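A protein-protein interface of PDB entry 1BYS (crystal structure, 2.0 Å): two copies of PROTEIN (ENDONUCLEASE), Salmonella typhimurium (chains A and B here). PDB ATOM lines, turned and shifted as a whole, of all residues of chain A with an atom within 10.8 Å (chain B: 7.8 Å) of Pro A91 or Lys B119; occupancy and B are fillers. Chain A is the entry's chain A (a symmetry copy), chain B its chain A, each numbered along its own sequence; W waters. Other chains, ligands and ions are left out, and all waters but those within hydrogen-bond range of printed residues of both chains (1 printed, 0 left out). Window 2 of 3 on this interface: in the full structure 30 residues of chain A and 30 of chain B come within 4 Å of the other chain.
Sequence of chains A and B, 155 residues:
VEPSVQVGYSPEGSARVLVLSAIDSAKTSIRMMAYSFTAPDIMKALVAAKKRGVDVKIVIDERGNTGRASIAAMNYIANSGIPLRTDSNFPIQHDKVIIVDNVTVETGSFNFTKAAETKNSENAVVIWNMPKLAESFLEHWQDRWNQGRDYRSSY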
ATOM      1  N   ALA A  34       2.728 -32.248 -20.902  1.00  0.00           N
ATOM      2  CA  ALA A  34       2.054 -33.340 -21.587  1.00  0.00           C
ATOM      3  C   ALA A  34       0.553 -33.280 -21.448  1.00  0.00           C
ATOM      4  O   ALA A  34       0.027 -32.748 -20.481  1.00  0.00           O
ATOM      5  CB  ALA A  34       2.550 -34.685 -21.062  1.00  0.00           C
ATOM      6  N   TYR A  35      -0.131 -33.828 -22.441  1.00  0.00           N
ATOM      7  CA  TYR A  35      -1.582 -33.935 -22.421  1.00  0.00           C
ATOM      8  C   TYR A  35      -1.683 -35.364 -21.843  1.00  0.00           C
ATOM      9  O   TYR A  35      -1.362 -35.570 -20.687  1.00  0.00           O
ATOM     10  CB  TYR A  35      -2.139 -33.856 -23.850  1.00  0.00           C
ATOM     11  CG  TYR A  35      -3.616 -34.199 -23.958  1.00  0.00           C
ATOM     12  CD1 TYR A  35      -4.547 -33.681 -23.060  1.00  0.00           C
ATOM     13  CD2 TYR A  35      -4.067 -35.060 -24.942  1.00  0.00           C
ATOM     14  CE1 TYR A  35      -5.892 -34.017 -23.141  1.00  0.00           C
ATOM     15  CE2 TYR A  35      -5.403 -35.406 -25.038  1.00  0.00           C
ATOM     16  CZ  TYR A  35      -6.324 -34.884 -24.141  1.00  0.00           C
ATOM     17  OH  TYR A  35      -7.675 -35.203 -24.272  1.00  0.00           O
ATOM     18  N   SER A  36      -2.096 -36.348 -22.629  1.00  0.00           N
ATOM     19  CA  SER A  36      -2.123 -37.716 -22.103  1.00  0.00           C
ATOM     20  C   SER A  36      -0.730 -38.072 -21.513  1.00  0.00           C
ATOM     21  O   SER A  36       0.297 -37.852 -22.156  1.00  0.00           O
ATOM     22  CB  SER A  36      -2.465 -38.689 -23.229  1.00  0.00           C
ATOM     23  OG  SER A  36      -3.692 -38.317 -23.821  1.00  0.00           O
ATOM     24  N   ILE A  60       1.238 -31.597 -16.507  1.00  0.00           N
ATOM     25  CA  ILE A  60       0.395 -32.307 -17.443  1.00  0.00           C
ATOM     26  C   ILE A  60      -1.048 -31.826 -17.394  1.00  0.00           C
ATOM     27  O   ILE A  60      -1.463 -31.145 -16.452  1.00  0.00           O
ATOM     28  CB  ILE A  60       0.455 -33.832 -17.172  1.00  0.00           C
ATOM     29  CG1 ILE A  60      -0.360 -34.178 -15.919  1.00  0.00           C
ATOM     30  CG2 ILE A  60       1.894 -34.258 -16.976  1.00  0.00           C
ATOM     31  CD1 ILE A  60      -0.286 -35.653 -15.525  1.00  0.00           C
ATOM     32  N   ASP A  61      -1.810 -32.155 -18.426  1.00  0.00           N
ATOM     33  CA  ASP A  61      -3.205 -31.765 -18.469  1.00  0.00           C
ATOM     34  C   ASP A  61      -3.957 -32.517 -17.379  1.00  0.00           C
ATOM     35  O   ASP A  61      -3.819 -33.727 -17.241  1.00  0.00           O
ATOM     36  CB  ASP A  61      -3.825 -32.102 -19.828  1.00  0.00           C
ATOM     37  CG  ASP A  61      -5.275 -31.670 -19.913  1.00  0.00           C
ATOM     38  OD1 ASP A  61      -5.546 -30.448 -19.918  1.00  0.00           O
ATOM     39  OD2 ASP A  61      -6.141 -32.557 -19.962  1.00  0.00           O
ATOM     40  N   GLU A  62      -4.779 -31.806 -16.623  1.00  0.00           N
ATOM     41  CA  GLU A  62      -5.518 -32.441 -15.550  1.00  0.00           C
ATOM     42  C   GLU A  62      -6.694 -33.300 -16.014  1.00  0.00           C
ATOM     43  O   GLU A  62      -6.752 -34.505 -15.736  1.00  0.00           O
ATOM     44  CB  GLU A  62      -6.013 -31.376 -14.590  1.00  0.00           C
ATOM     45  CG  GLU A  62      -6.339 -31.926 -13.237  1.00  0.00           C
ATOM     46  CD  GLU A  62      -7.602 -31.329 -12.689  1.00  0.00           C
ATOM     47  OE1 GLU A  62      -8.697 -31.662 -13.203  1.00  0.00           O
ATOM     48  OE2 GLU A  62      -7.488 -30.520 -11.752  1.00  0.00           O
ATOM     49  N   ARG A  63      -7.626 -32.682 -16.738  1.00  0.00           N
ATOM     50  CA  ARG A  63      -8.816 -33.394 -17.205  1.00  0.00           C
ATOM     51  C   ARG A  63      -8.575 -34.654 -18.055  1.00  0.00           C
ATOM     52  O   ARG A  63      -9.347 -35.610 -17.989  1.00  0.00           O
ATOM     53  CB  ARG A  63      -9.726 -32.425 -17.968  1.00  0.00           C
ATOM     54  CG  ARG A  63     -10.302 -31.312 -17.107  1.00  0.00           C
ATOM     55  CD  ARG A  63     -11.574 -30.775 -17.727  1.00  0.00           C
ATOM     56  NE  ARG A  63     -12.018 -31.645 -18.811  1.00  0.00           N
ATOM     57  CZ  ARG A  63     -11.986 -31.320 -20.099  1.00  0.00           C
ATOM     58  NH1 ARG A  63     -11.530 -30.129 -20.479  1.00  0.00           N
ATOM     59  NH2 ARG A  63     -12.392 -32.196 -21.011  1.00  0.00           N
ATOM     60  N   GLY A  64      -7.518 -34.649 -18.861  1.00  0.00           N
ATOM     61  CA  GLY A  64      -7.243 -35.812 -19.685  1.00  0.00           C
ATOM     62  C   GLY A  64      -6.365 -36.848 -18.990  1.00  0.00           C
ATOM     63  O   GLY A  64      -5.884 -37.793 -19.619  1.00  0.00           O
ATOM     64  N   ASN A  65      -6.159 -36.691 -17.689  1.00  0.00           N
ATOM     65  CA  ASN A  65      -5.326 -37.643 -16.982  1.00  0.00           C
ATOM     66  C   ASN A  65      -5.985 -38.211 -15.721  1.00  0.00           C
ATOM     67  O   ASN A  65      -5.390 -38.235 -14.641  1.00  0.00           O
ATOM     68  CB  ASN A  65      -3.973 -36.999 -16.646  1.00  0.00           C
ATOM     69  CG  ASN A  65      -3.007 -37.017 -17.833  1.00  0.00           C
ATOM     70  OD1 ASN A  65      -2.704 -38.068 -18.398  1.00  0.00           O
ATOM     71  ND2 ASN A  65      -2.523 -35.852 -18.206  1.00  0.00           N
ATOM     72  N   ASP A  87      -2.654 -29.276 -14.649  1.00  0.00           N
ATOM     73  CA  ASP A  87      -3.086 -27.938 -15.047  1.00  0.00           C
ATOM     74  C   ASP A  87      -4.459 -28.075 -15.676  1.00  0.00           C
ATOM     75  O   ASP A  87      -4.621 -28.796 -16.656  1.00  0.00           O
ATOM     76  CB  ASP A  87      -2.083 -27.343 -16.059  1.00  0.00           C
ATOM     77  CG  ASP A  87      -2.521 -25.970 -16.624  1.00  0.00           C
ATOM     78  OD1 ASP A  87      -3.363 -25.281 -16.015  1.00  0.00           O
ATOM     79  OD2 ASP A  87      -2.000 -25.581 -17.693  1.00  0.00           O
ATOM     80  N   SER A  88      -5.446 -27.395 -15.103  1.00  0.00           N
ATOM     81  CA  SER A  88      -6.811 -27.453 -15.625  1.00  0.00           C
ATOM     82  C   SER A  88      -7.297 -26.090 -16.074  1.00  0.00           C
ATOM     83  O   SER A  88      -8.471 -25.922 -16.366  1.00  0.00           O
ATOM     84  CB  SER A  88      -7.777 -27.965 -14.557  1.00  0.00           C
ATOM     85  OG  SER A  88      -7.858 -27.036 -13.490  1.00  0.00           O
ATOM     86  N   ASN A  89      -6.395 -25.123 -16.130  1.00  0.00           N
ATOM     87  CA  ASN A  89      -6.794 -23.796 -16.516  1.00  0.00           C
ATOM     88  C   ASN A  89      -7.074 -23.638 -18.010  1.00  0.00           C
ATOM     89  O   ASN A  89      -7.571 -22.598 -18.435  1.00  0.00           O
ATOM     90  CB  ASN A  89      -5.760 -22.794 -16.028  1.00  0.00           C
ATOM     91  CG  ASN A  89      -5.855 -22.555 -14.522  1.00  0.00           C
ATOM     92  OD1 ASN A  89      -6.821 -22.981 -13.876  1.00  0.00           O
ATOM     93  ND2 ASN A  89      -4.858 -21.883 -13.959  1.00  0.00           N
ATOM     94  N   PHE A  90      -6.774 -24.664 -18.802  1.00  0.00           N
ATOM     95  CA  PHE A  90      -7.041 -24.623 -20.247  1.00  0.00           C
ATOM     96  C   PHE A  90      -7.961 -25.800 -20.568  1.00  0.00           C
ATOM     97  O   PHE A  90      -7.785 -26.894 -20.030  1.00  0.00           O
ATOM     98  CB  PHE A  90      -5.734 -24.753 -21.059  1.00  0.00           C
ATOM     99  CG  PHE A  90      -4.693 -23.714 -20.719  1.00  0.00           C
ATOM    100  CD1 PHE A  90      -3.780 -23.942 -19.690  1.00  0.00           C
ATOM    101  CD2 PHE A  90      -4.652 -22.498 -21.400  1.00  0.00           C
ATOM    102  CE1 PHE A  90      -2.848 -22.979 -19.337  1.00  0.00           C
ATOM    103  CE2 PHE A  90      -3.721 -21.525 -21.054  1.00  0.00           C
ATOM    104  CZ  PHE A  90      -2.814 -21.760 -20.021  1.00  0.00           C
ATOM    105  N   PRO A  91      -8.965 -25.598 -21.434  1.00  0.00           N
ATOM    106  CA  PRO A  91      -9.836 -26.738 -21.729  1.00  0.00           C
ATOM    107  C   PRO A  91      -8.970 -27.968 -21.959  1.00  0.00           C
ATOM    108  O   PRO A  91      -9.350 -29.097 -21.637  1.00  0.00           O
ATOM    109  CB  PRO A  91     -10.595 -26.288 -22.975  1.00  0.00           C
ATOM    110  CG  PRO A  91     -10.681 -24.802 -22.803  1.00  0.00           C
ATOM    111  CD  PRO A  91      -9.376 -24.382 -22.159  1.00  0.00           C
ATOM    112  N   ILE A  92      -7.811 -27.724 -22.557  1.00  0.00           N
ATOM    113  CA  ILE A  92      -6.820 -28.760 -22.800  1.00  0.00           C
ATOM    114  C   ILE A  92      -5.405 -28.192 -22.857  1.00  0.00           C
ATOM    115  O   ILE A  92      -5.095 -27.351 -23.732  1.00  0.00           O
ATOM    116  CB  ILE A  92      -7.012 -29.526 -24.143  1.00  0.00           C
ATOM    117  CG1 ILE A  92      -8.444 -30.032 -24.309  1.00  0.00           C
ATOM    118  CG2 ILE A  92      -6.055 -30.723 -24.173  1.00  0.00           C
ATOM    119  CD1 ILE A  92      -8.617 -30.818 -25.575  1.00  0.00           C
ATOM    120  N   GLN A  93      -4.550 -28.601 -21.920  1.00  0.00           N
ATOM    121  CA  GLN A  93      -3.159 -28.188 -21.985  1.00  0.00           C
ATOM    122  C   GLN A  93      -2.725 -29.261 -22.975  1.00  0.00           C
ATOM    123  O   GLN A  93      -2.444 -30.407 -22.586  1.00  0.00           O
ATOM    124  CB  GLN A  93      -2.429 -28.364 -20.655  1.00  0.00           C
ATOM    125  CG  GLN A  93      -1.039 -27.719 -20.694  1.00  0.00           C
ATOM    126  CD  GLN A  93      -0.097 -28.233 -19.604  1.00  0.00           C
ATOM    127  OE1 GLN A  93       0.622 -29.209 -19.790  1.00  0.00           O
ATOM    128  NE2 GLN A  93      -0.094 -27.564 -18.466  1.00  0.00           N
ATOM    129  N   HIS A  94      -2.700 -28.880 -24.252  1.00  0.00           N
ATOM    130  CA  HIS A  94      -2.417 -29.785 -25.364  1.00  0.00           C
ATOM    131  C   HIS A  94      -0.973 -30.062 -25.830  1.00  0.00           C
ATOM    132  O   HIS A  94      -0.758 -30.963 -26.628  1.00  0.00           O
ATOM    133  CB  HIS A  94      -3.262 -29.321 -26.550  1.00  0.00           C
ATOM    134  CG  HIS A  94      -3.540 -30.390 -27.553  1.00  0.00           C
ATOM    135  ND1 HIS A  94      -2.889 -30.467 -28.768  1.00  0.00           N
ATOM    136  CD2 HIS A  94      -4.388 -31.445 -27.513  1.00  0.00           C
ATOM    137  CE1 HIS A  94      -3.323 -31.520 -29.436  1.00  0.00           C
ATOM    138  NE2 HIS A  94      -4.232 -32.127 -28.693  1.00  0.00           N
ATOM    139  N   ASP A  95      -0.007 -29.295 -25.345  1.00  0.00           N
ATOM    140  CA  ASP A  95       1.410 -29.481 -25.708  1.00  0.00           C
ATOM    141  C   ASP A  95       1.987 -30.864 -25.388  1.00  0.00           C
ATOM    142  O   ASP A  95       1.618 -31.476 -24.378  1.00  0.00           O
ATOM    143  CB  ASP A  95       2.293 -28.443 -24.987  1.00  0.00           C
ATOM    144  CG  ASP A  95       1.735 -27.026 -25.069  1.00  0.00           C
ATOM    145  OD1 ASP A  95       0.871 -26.660 -24.233  1.00  0.00           O
ATOM    146  OD2 ASP A  95       2.169 -26.276 -25.966  1.00  0.00           O
ATOM    147  N   HIS A 140       6.915 -20.757 -21.735  1.00  0.00           N
ATOM    148  CA  HIS A 140       5.636 -21.402 -22.035  1.00  0.00           C
ATOM    149  C   HIS A 140       5.384 -22.448 -20.947  1.00  0.00           C
ATOM    150  O   HIS A 140       4.316 -22.490 -20.347  1.00  0.00           O
ATOM    151  CB  HIS A 140       5.734 -22.076 -23.410  1.00  0.00           C
ATOM    152  CG  HIS A 140       4.455 -22.686 -23.908  1.00  0.00           C
ATOM    153  ND1 HIS A 140       3.266 -21.992 -23.969  1.00  0.00           N
ATOM    154  CD2 HIS A 140       4.208 -23.892 -24.470  1.00  0.00           C
ATOM    155  CE1 HIS A 140       2.342 -22.741 -24.551  1.00  0.00           C
ATOM    156  NE2 HIS A 140       2.893 -23.900 -24.864  1.00  0.00           N
ATOM    157  N   ASP A 143       4.761 -20.806 -17.423  1.00  0.00           N
ATOM    158  CA  ASP A 143       3.451 -20.172 -17.258  1.00  0.00           C
ATOM    159  C   ASP A 143       2.401 -21.213 -16.901  1.00  0.00           C
ATOM    160  O   ASP A 143       1.542 -20.987 -16.049  1.00  0.00           O
ATOM    161  CB  ASP A 143       3.025 -19.460 -18.542  1.00  0.00           C
ATOM    162  CG  ASP A 143       1.710 -18.727 -18.384  1.00  0.00           C
ATOM    163  OD1 ASP A 143       1.729 -17.587 -17.886  1.00  0.00           O
ATOM    164  OD2 ASP A 143       0.659 -19.287 -18.748  1.00  0.00           O
ATOM    165  N   ARG A 144       2.463 -22.360 -17.562  1.00  0.00           N
ATOM    166  CA  ARG A 144       1.510 -23.427 -17.290  1.00  0.00           C
ATOM    167  C   ARG A 144       1.796 -24.094 -15.926  1.00  0.00           C
ATOM    168  O   ARG A 144       0.877 -24.371 -15.151  1.00  0.00           O
ATOM    169  CB  ARG A 144       1.585 -24.462 -18.412  1.00  0.00           C
ATOM    170  CG  ARG A 144       0.732 -24.135 -19.637  1.00  0.00           C
ATOM    171  CD  ARG A 144       0.903 -22.695 -20.118  1.00  0.00           C
ATOM    172  NE  ARG A 144       0.369 -22.530 -21.480  1.00  0.00           N
ATOM    173  CZ  ARG A 144       0.258 -21.367 -22.125  1.00  0.00           C
ATOM    174  NH1 ARG A 144       0.640 -20.234 -21.541  1.00  0.00           N
ATOM    175  NH2 ARG A 144      -0.191 -21.344 -23.383  1.00  0.00           N
ATOM    176  N   GLN A 147       0.560 -22.302 -12.832  1.00  0.00           N
ATOM    177  CA  GLN A 147      -0.861 -22.354 -12.500  1.00  0.00           C
ATOM    178  C   GLN A 147      -1.349 -23.778 -12.300  1.00  0.00           C
ATOM    179  O   GLN A 147      -2.552 -24.032 -12.326  1.00  0.00           O
ATOM    180  CB  GLN A 147      -1.700 -21.675 -13.590  1.00  0.00           C
ATOM    181  CG  GLN A 147      -1.377 -22.133 -14.998  1.00  0.00           C
ATOM    182  CD  GLN A 147      -1.860 -21.135 -16.031  1.00  0.00           C
ATOM    183  OE1 GLN A 147      -2.979 -20.635 -15.940  1.00  0.00           O
ATOM    184  NE2 GLN A 147      -1.020 -20.837 -17.010  1.00  0.00           N
ATOM    185  N   SER B  10      -0.574 -21.041 -28.187  1.00  0.00           N
ATOM    186  CA  SER B  10      -1.998 -20.815 -27.990  1.00  0.00           C
ATOM    187  C   SER B  10      -2.247 -21.022 -26.498  1.00  0.00           C
ATOM    188  O   SER B  10      -1.484 -21.717 -25.830  1.00  0.00           O
ATOM    189  CB  SER B  10      -2.843 -21.810 -28.778  1.00  0.00           C
ATOM    190  OG  SER B  10      -2.619 -21.649 -30.158  1.00  0.00           O
ATOM    191  N   PRO B  11      -3.292 -20.398 -25.948  1.00  0.00           N
ATOM    192  CA  PRO B  11      -4.231 -19.521 -26.668  1.00  0.00           C
ATOM    193  C   PRO B  11      -3.679 -18.088 -26.874  1.00  0.00           C
ATOM    194  O   PRO B  11      -4.417 -17.188 -27.259  1.00  0.00           O
ATOM    195  CB  PRO B  11      -5.468 -19.524 -25.769  1.00  0.00           C
ATOM    196  CG  PRO B  11      -4.875 -19.664 -24.359  1.00  0.00           C
ATOM    197  CD  PRO B  11      -3.649 -20.554 -24.521  1.00  0.00           C
ATOM    198  N   GLU B  12      -2.387 -17.885 -26.618  1.00  0.00           N
ATOM    199  CA  GLU B  12      -1.765 -16.573 -26.768  1.00  0.00           C
ATOM    200  C   GLU B  12      -2.089 -15.879 -28.097  1.00  0.00           C
ATOM    201  O   GLU B  12      -2.292 -14.666 -28.147  1.00  0.00           O
ATOM    202  CB  GLU B  12      -0.245 -16.710 -26.638  1.00  0.00           C
ATOM    203  CG  GLU B  12       0.272 -16.658 -25.209  1.00  0.00           C
ATOM    204  CD  GLU B  12       0.074 -17.972 -24.452  1.00  0.00           C
ATOM    205  OE1 GLU B  12      -0.485 -18.935 -25.035  1.00  0.00           O
ATOM    206  OE2 GLU B  12       0.482 -18.034 -23.267  1.00  0.00           O
ATOM    207  N   THR B 113      -7.771 -26.206 -35.918  1.00  0.00           N
ATOM    208  CA  THR B 113      -9.130 -25.959 -35.429  1.00  0.00           C
ATOM    209  C   THR B 113      -9.190 -24.647 -34.634  1.00  0.00           C
ATOM    210  O   THR B 113      -8.162 -24.140 -34.178  1.00  0.00           O
ATOM    211  CB  THR B 113      -9.600 -27.074 -34.468  1.00  0.00           C
ATOM    212  OG1 THR B 113      -8.875 -26.949 -33.234  1.00  0.00           O
ATOM    213  CG2 THR B 113      -9.378 -28.466 -35.067  1.00  0.00           C
ATOM    214  N   LYS B 114     -10.390 -24.106 -34.445  1.00  0.00           N
ATOM    215  CA  LYS B 114     -10.531 -22.876 -33.675  1.00  0.00           C
ATOM    216  C   LYS B 114     -10.149 -23.105 -32.195  1.00  0.00           C
ATOM    217  O   LYS B 114      -9.622 -22.209 -31.536  1.00  0.00           O
ATOM    218  CB  LYS B 114     -11.974 -22.352 -33.789  1.00  0.00           C
ATOM    219  CG  LYS B 114     -12.400 -22.009 -35.232  1.00  0.00           C
ATOM    220  CD  LYS B 114     -11.238 -21.436 -36.067  1.00  0.00           C
ATOM    221  CE  LYS B 114     -11.609 -20.089 -36.739  1.00  0.00           C
ATOM    222  NZ  LYS B 114     -10.767 -19.732 -37.934  1.00  0.00           N
ATOM    223  N   ALA B 115     -10.402 -24.311 -31.689  1.00  0.00           N
ATOM    224  CA  ALA B 115     -10.061 -24.643 -30.303  1.00  0.00           C
ATOM    225  C   ALA B 115      -8.537 -24.565 -30.109  1.00  0.00           C
ATOM    226  O   ALA B 115      -8.056 -24.093 -29.074  1.00  0.00           O
ATOM    227  CB  ALA B 115     -10.567 -26.055 -29.956  1.00  0.00           C
ATOM    228  N   ALA B 116      -7.792 -25.021 -31.112  1.00  0.00           N
ATOM    229  CA  ALA B 116      -6.337 -24.984 -31.052  1.00  0.00           C
ATOM    230  C   ALA B 116      -5.832 -23.552 -31.247  1.00  0.00           C
ATOM    231  O   ALA B 116      -4.717 -23.220 -30.848  1.00  0.00           O
ATOM    232  CB  ALA B 116      -5.753 -25.882 -32.124  1.00  0.00           C
ATOM    233  N   GLU B 117      -6.656 -22.698 -31.847  1.00  0.00           N
ATOM    234  CA  GLU B 117      -6.240 -21.316 -32.073  1.00  0.00           C
ATOM    235  C   GLU B 117      -6.479 -20.388 -30.877  1.00  0.00           C
ATOM    236  O   GLU B 117      -5.637 -19.542 -30.553  1.00  0.00           O
ATOM    237  CB  GLU B 117      -6.959 -20.758 -33.309  1.00  0.00           C
ATOM    238  CG  GLU B 117      -6.381 -21.274 -34.616  1.00  0.00           C
ATOM    239  CD  GLU B 117      -7.255 -20.956 -35.838  1.00  0.00           C
ATOM    240  OE1 GLU B 117      -8.401 -20.482 -35.663  1.00  0.00           O
ATOM    241  OE2 GLU B 117      -6.783 -21.181 -36.976  1.00  0.00           O
ATOM    242  N   THR B 118      -7.607 -20.565 -30.201  1.00  0.00           N
ATOM    243  CA  THR B 118      -7.950 -19.683 -29.092  1.00  0.00           C
ATOM    244  C   THR B 118      -8.313 -20.268 -27.718  1.00  0.00           C
ATOM    245  O   THR B 118      -8.687 -19.508 -26.833  1.00  0.00           O
ATOM    246  CB  THR B 118      -9.130 -18.766 -29.496  1.00  0.00           C
ATOM    247  OG1 THR B 118     -10.328 -19.552 -29.574  1.00  0.00           O
ATOM    248  CG2 THR B 118      -8.868 -18.120 -30.863  1.00  0.00           C
ATOM    249  N   LYS B 119      -8.207 -21.574 -27.517  1.00  0.00           N
ATOM    250  CA  LYS B 119      -8.581 -22.129 -26.212  1.00  0.00           C
ATOM    251  C   LYS B 119      -7.560 -23.043 -25.533  1.00  0.00           C
ATOM    252  O   LYS B 119      -7.219 -22.858 -24.356  1.00  0.00           O
ATOM    253  CB  LYS B 119      -9.918 -22.871 -26.355  1.00  0.00           C
ATOM    254  CG  LYS B 119     -10.951 -22.070 -27.168  1.00  0.00           C
ATOM    255  CD  LYS B 119     -12.338 -22.661 -27.035  1.00  0.00           C
ATOM    256  CE  LYS B 119     -12.672 -23.581 -28.215  1.00  0.00           C
ATOM    257  NZ  LYS B 119     -13.562 -22.920 -29.219  1.00  0.00           N
ATOM    258  N   ASN B 120      -7.094 -24.042 -26.266  1.00  0.00           N
ATOM    259  CA  ASN B 120      -6.122 -24.982 -25.725  1.00  0.00           C
ATOM    260  C   ASN B 120      -4.748 -24.345 -25.594  1.00  0.00           C
ATOM    261  O   ASN B 120      -4.454 -23.313 -26.230  1.00  0.00           O
ATOM    262  CB  ASN B 120      -5.975 -26.186 -26.652  1.00  0.00           C
ATOM    263  CG  ASN B 120      -7.272 -26.906 -26.884  1.00  0.00           C
ATOM    264  OD1 ASN B 120      -8.220 -26.781 -26.106  1.00  0.00           O
ATOM    265  ND2 ASN B 120      -7.327 -27.671 -27.959  1.00  0.00           N
ATOM    266  N   SER B 121      -3.899 -24.942 -24.764  1.00  0.00           N
ATOM    267  CA  SER B 121      -2.538 -24.446 -24.669  1.00  0.00           C
ATOM    268  C   SER B 121      -1.888 -25.255 -25.788  1.00  0.00           C
ATOM    269  O   SER B 121      -2.090 -26.471 -25.864  1.00  0.00           O
ATOM    270  CB  SER B 121      -1.882 -24.792 -23.330  1.00  0.00           C
ATOM    271  OG  SER B 121      -0.476 -24.604 -23.433  1.00  0.00           O
ATOM    272  N   GLU B 122      -1.159 -24.597 -26.685  1.00  0.00           N
ATOM    273  CA  GLU B 122      -0.522 -25.292 -27.804  1.00  0.00           C
ATOM    274  C   GLU B 122       0.777 -24.650 -28.189  1.00  0.00           C
ATOM    275  O   GLU B 122       1.094 -23.550 -27.760  1.00  0.00           O
ATOM    276  CB  GLU B 122      -1.406 -25.256 -29.071  1.00  0.00           C
ATOM    277  CG  GLU B 122      -2.868 -25.578 -28.874  1.00  0.00           C
ATOM    278  CD  GLU B 122      -3.166 -27.034 -29.094  1.00  0.00           C
ATOM    279  OE1 GLU B 122      -2.217 -27.857 -29.152  1.00  0.00           O
ATOM    280  OE2 GLU B 122      -4.361 -27.352 -29.198  1.00  0.00           O
HETATM  281  O   HOH W   1       3.281 -19.418 -23.810  1.00  0.00           O
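The backbone carbonyl oxygen (O) of Ser B10 lies within hydrogen-bond range of the guanidinium group (NH2) of Arg A144 (2.8 Å).
OE2 of Glu B12 is in salt-bridge range of NH1 of Arg A144 (2.8 Å).
O of Ile A92 sits at hydrogen-bond distance from N of Ser B121 (2.9 Å).
The backbone carbonyl oxygen (O) of Ser B121 lies within hydrogen-bond range of the backbone NH (N) of His A94.
The side-chain hydroxyl of Ser B121 sits at hydrogen-bond distance from the side-chain carboxylate of Asp A95 (2.6 Å).
OG of Ser B121 sits at hydrogen-bond distance from NE of Arg A144 (3.0 Å).
OE1 of Glu B122 sits at hydrogen-bond distance from ND1 of His A94, 2.7 Å away.
The backbone carbonyl oxygen (O) of Glu B122 lies within hydrogen-bond range of a ring nitrogen (NE2) of His A140, 3.4 Å away.
The side-chain carboxylate of Asp A95 sits close to the backbone carbonyl oxygen of Glu B122 (3.4 Å).
The side-chain amide nitrogen of Asn B120 lies within hydrogen-bond range of the side-chain carboxylate of Glu B122 (3.2 Å).
OD1 of Asp A61 is in hydrogen-bond range of N of Gln A93 (2.9 Å).
The backbone carbonyl oxygen (O) of Pro A91 lies within hydrogen-bond range of the guanidinium group (NH1) of Arg A63 (2.7 Å).
The side-chain carboxylate of Asp A87 sits at hydrogen-bond distance from the side-chain amide nitrogen of Gln A93, 2.9 Å away.
A ring nitrogen (NE2) of His A140 is in hydrogen-bond range of the side-chain carboxylate of Asp A95, 2.7 Å away.
The guanidinium group (NH1) of Arg A144 lies within salt-bridge range of the side-chain carboxylate (OD2) of Asp A143.
Among the printed residues, pairs that only touch across the chains: Phe A90 with Pro B11, Phe A90 with Lys B119, Phe A90 with Ser B121, Pro A91 with Lys B119, Pro A91 with Asn B120, Ile A92 with Asn B120, Gln A93 with Ser B121, His A140 with Ser B121 and Arg A144 with Pro B11.
Of the printed residues of chain B, Phe A90 touches Pro B11 (3.6 Å), Lys B119 (3.9 Å) and Ser B121 (3.99 Å).
Pro A91 touches just these residues of chain B: Lys B119 and Asn B120.
Of the printed residues of chain B, Ile A92 touches Asn B120 (3.3 Å) and Ser B121 (2.9 Å).
Of the printed residues of chain B, His A94 touches Ser B121 and Glu B122.
Of the printed residues of chain B, Asp A95 touches Ser B121 (2.6 Å) and Glu B122 (3.1 Å).
Printed residues of chain A within 4 Å of Pro B11: Phe A90 (3.6 Å) and Arg A144 (3.7 Å).
Lys B114 touches none of the printed residues of chain A.
No residue of chain A comes within 4 Å of Ala B115.
No residue of chain A comes within 4 Å of Thr B118.
Lys B119 touches two residues of chain A.
Of the printed residues of chain A, Ser B121 touches Phe A90, Ile A92, Gln A93, His A94, Asp A95, His A140 and Arg A144.
The nearest residue of chain A that does not touch Lys B119 is Ile A92 (5.0 Å).
The nearest printed residue of chain B that does not touch Arg A144 is Glu B122 (4.7 Å).
Printed residues of chain B that touch a printed residue of chain A: Ser B10, Pro B11, Glu B12, Lys B119, Asn B120, Ser B121 and Glu B122.
Hydrophobic or aromatic side chains of chain B that line the printed part of chain A: Pro B11.
Of the 22 printed residues of chain A, 8 touch a printed residue of chain B.
Printed residues of chain A that touch a printed residue of chain B: Phe A90, Pro A91, Ile A92, Gln A93, His A94, Asp A95, His A140 and Arg A144.
Hydrophobic or aromatic side chains of chain A that line the printed part of chain B: Phe A90, Pro A91, Ile A92, His A94 and His A140.
No position is printed for both chains.
Water W1 lies within hydrogen-bond range of a ring nitrogen (ND1) of His A140 (2.6 Å) and the side-chain carboxylate of Glu B12 (3.2 Å).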
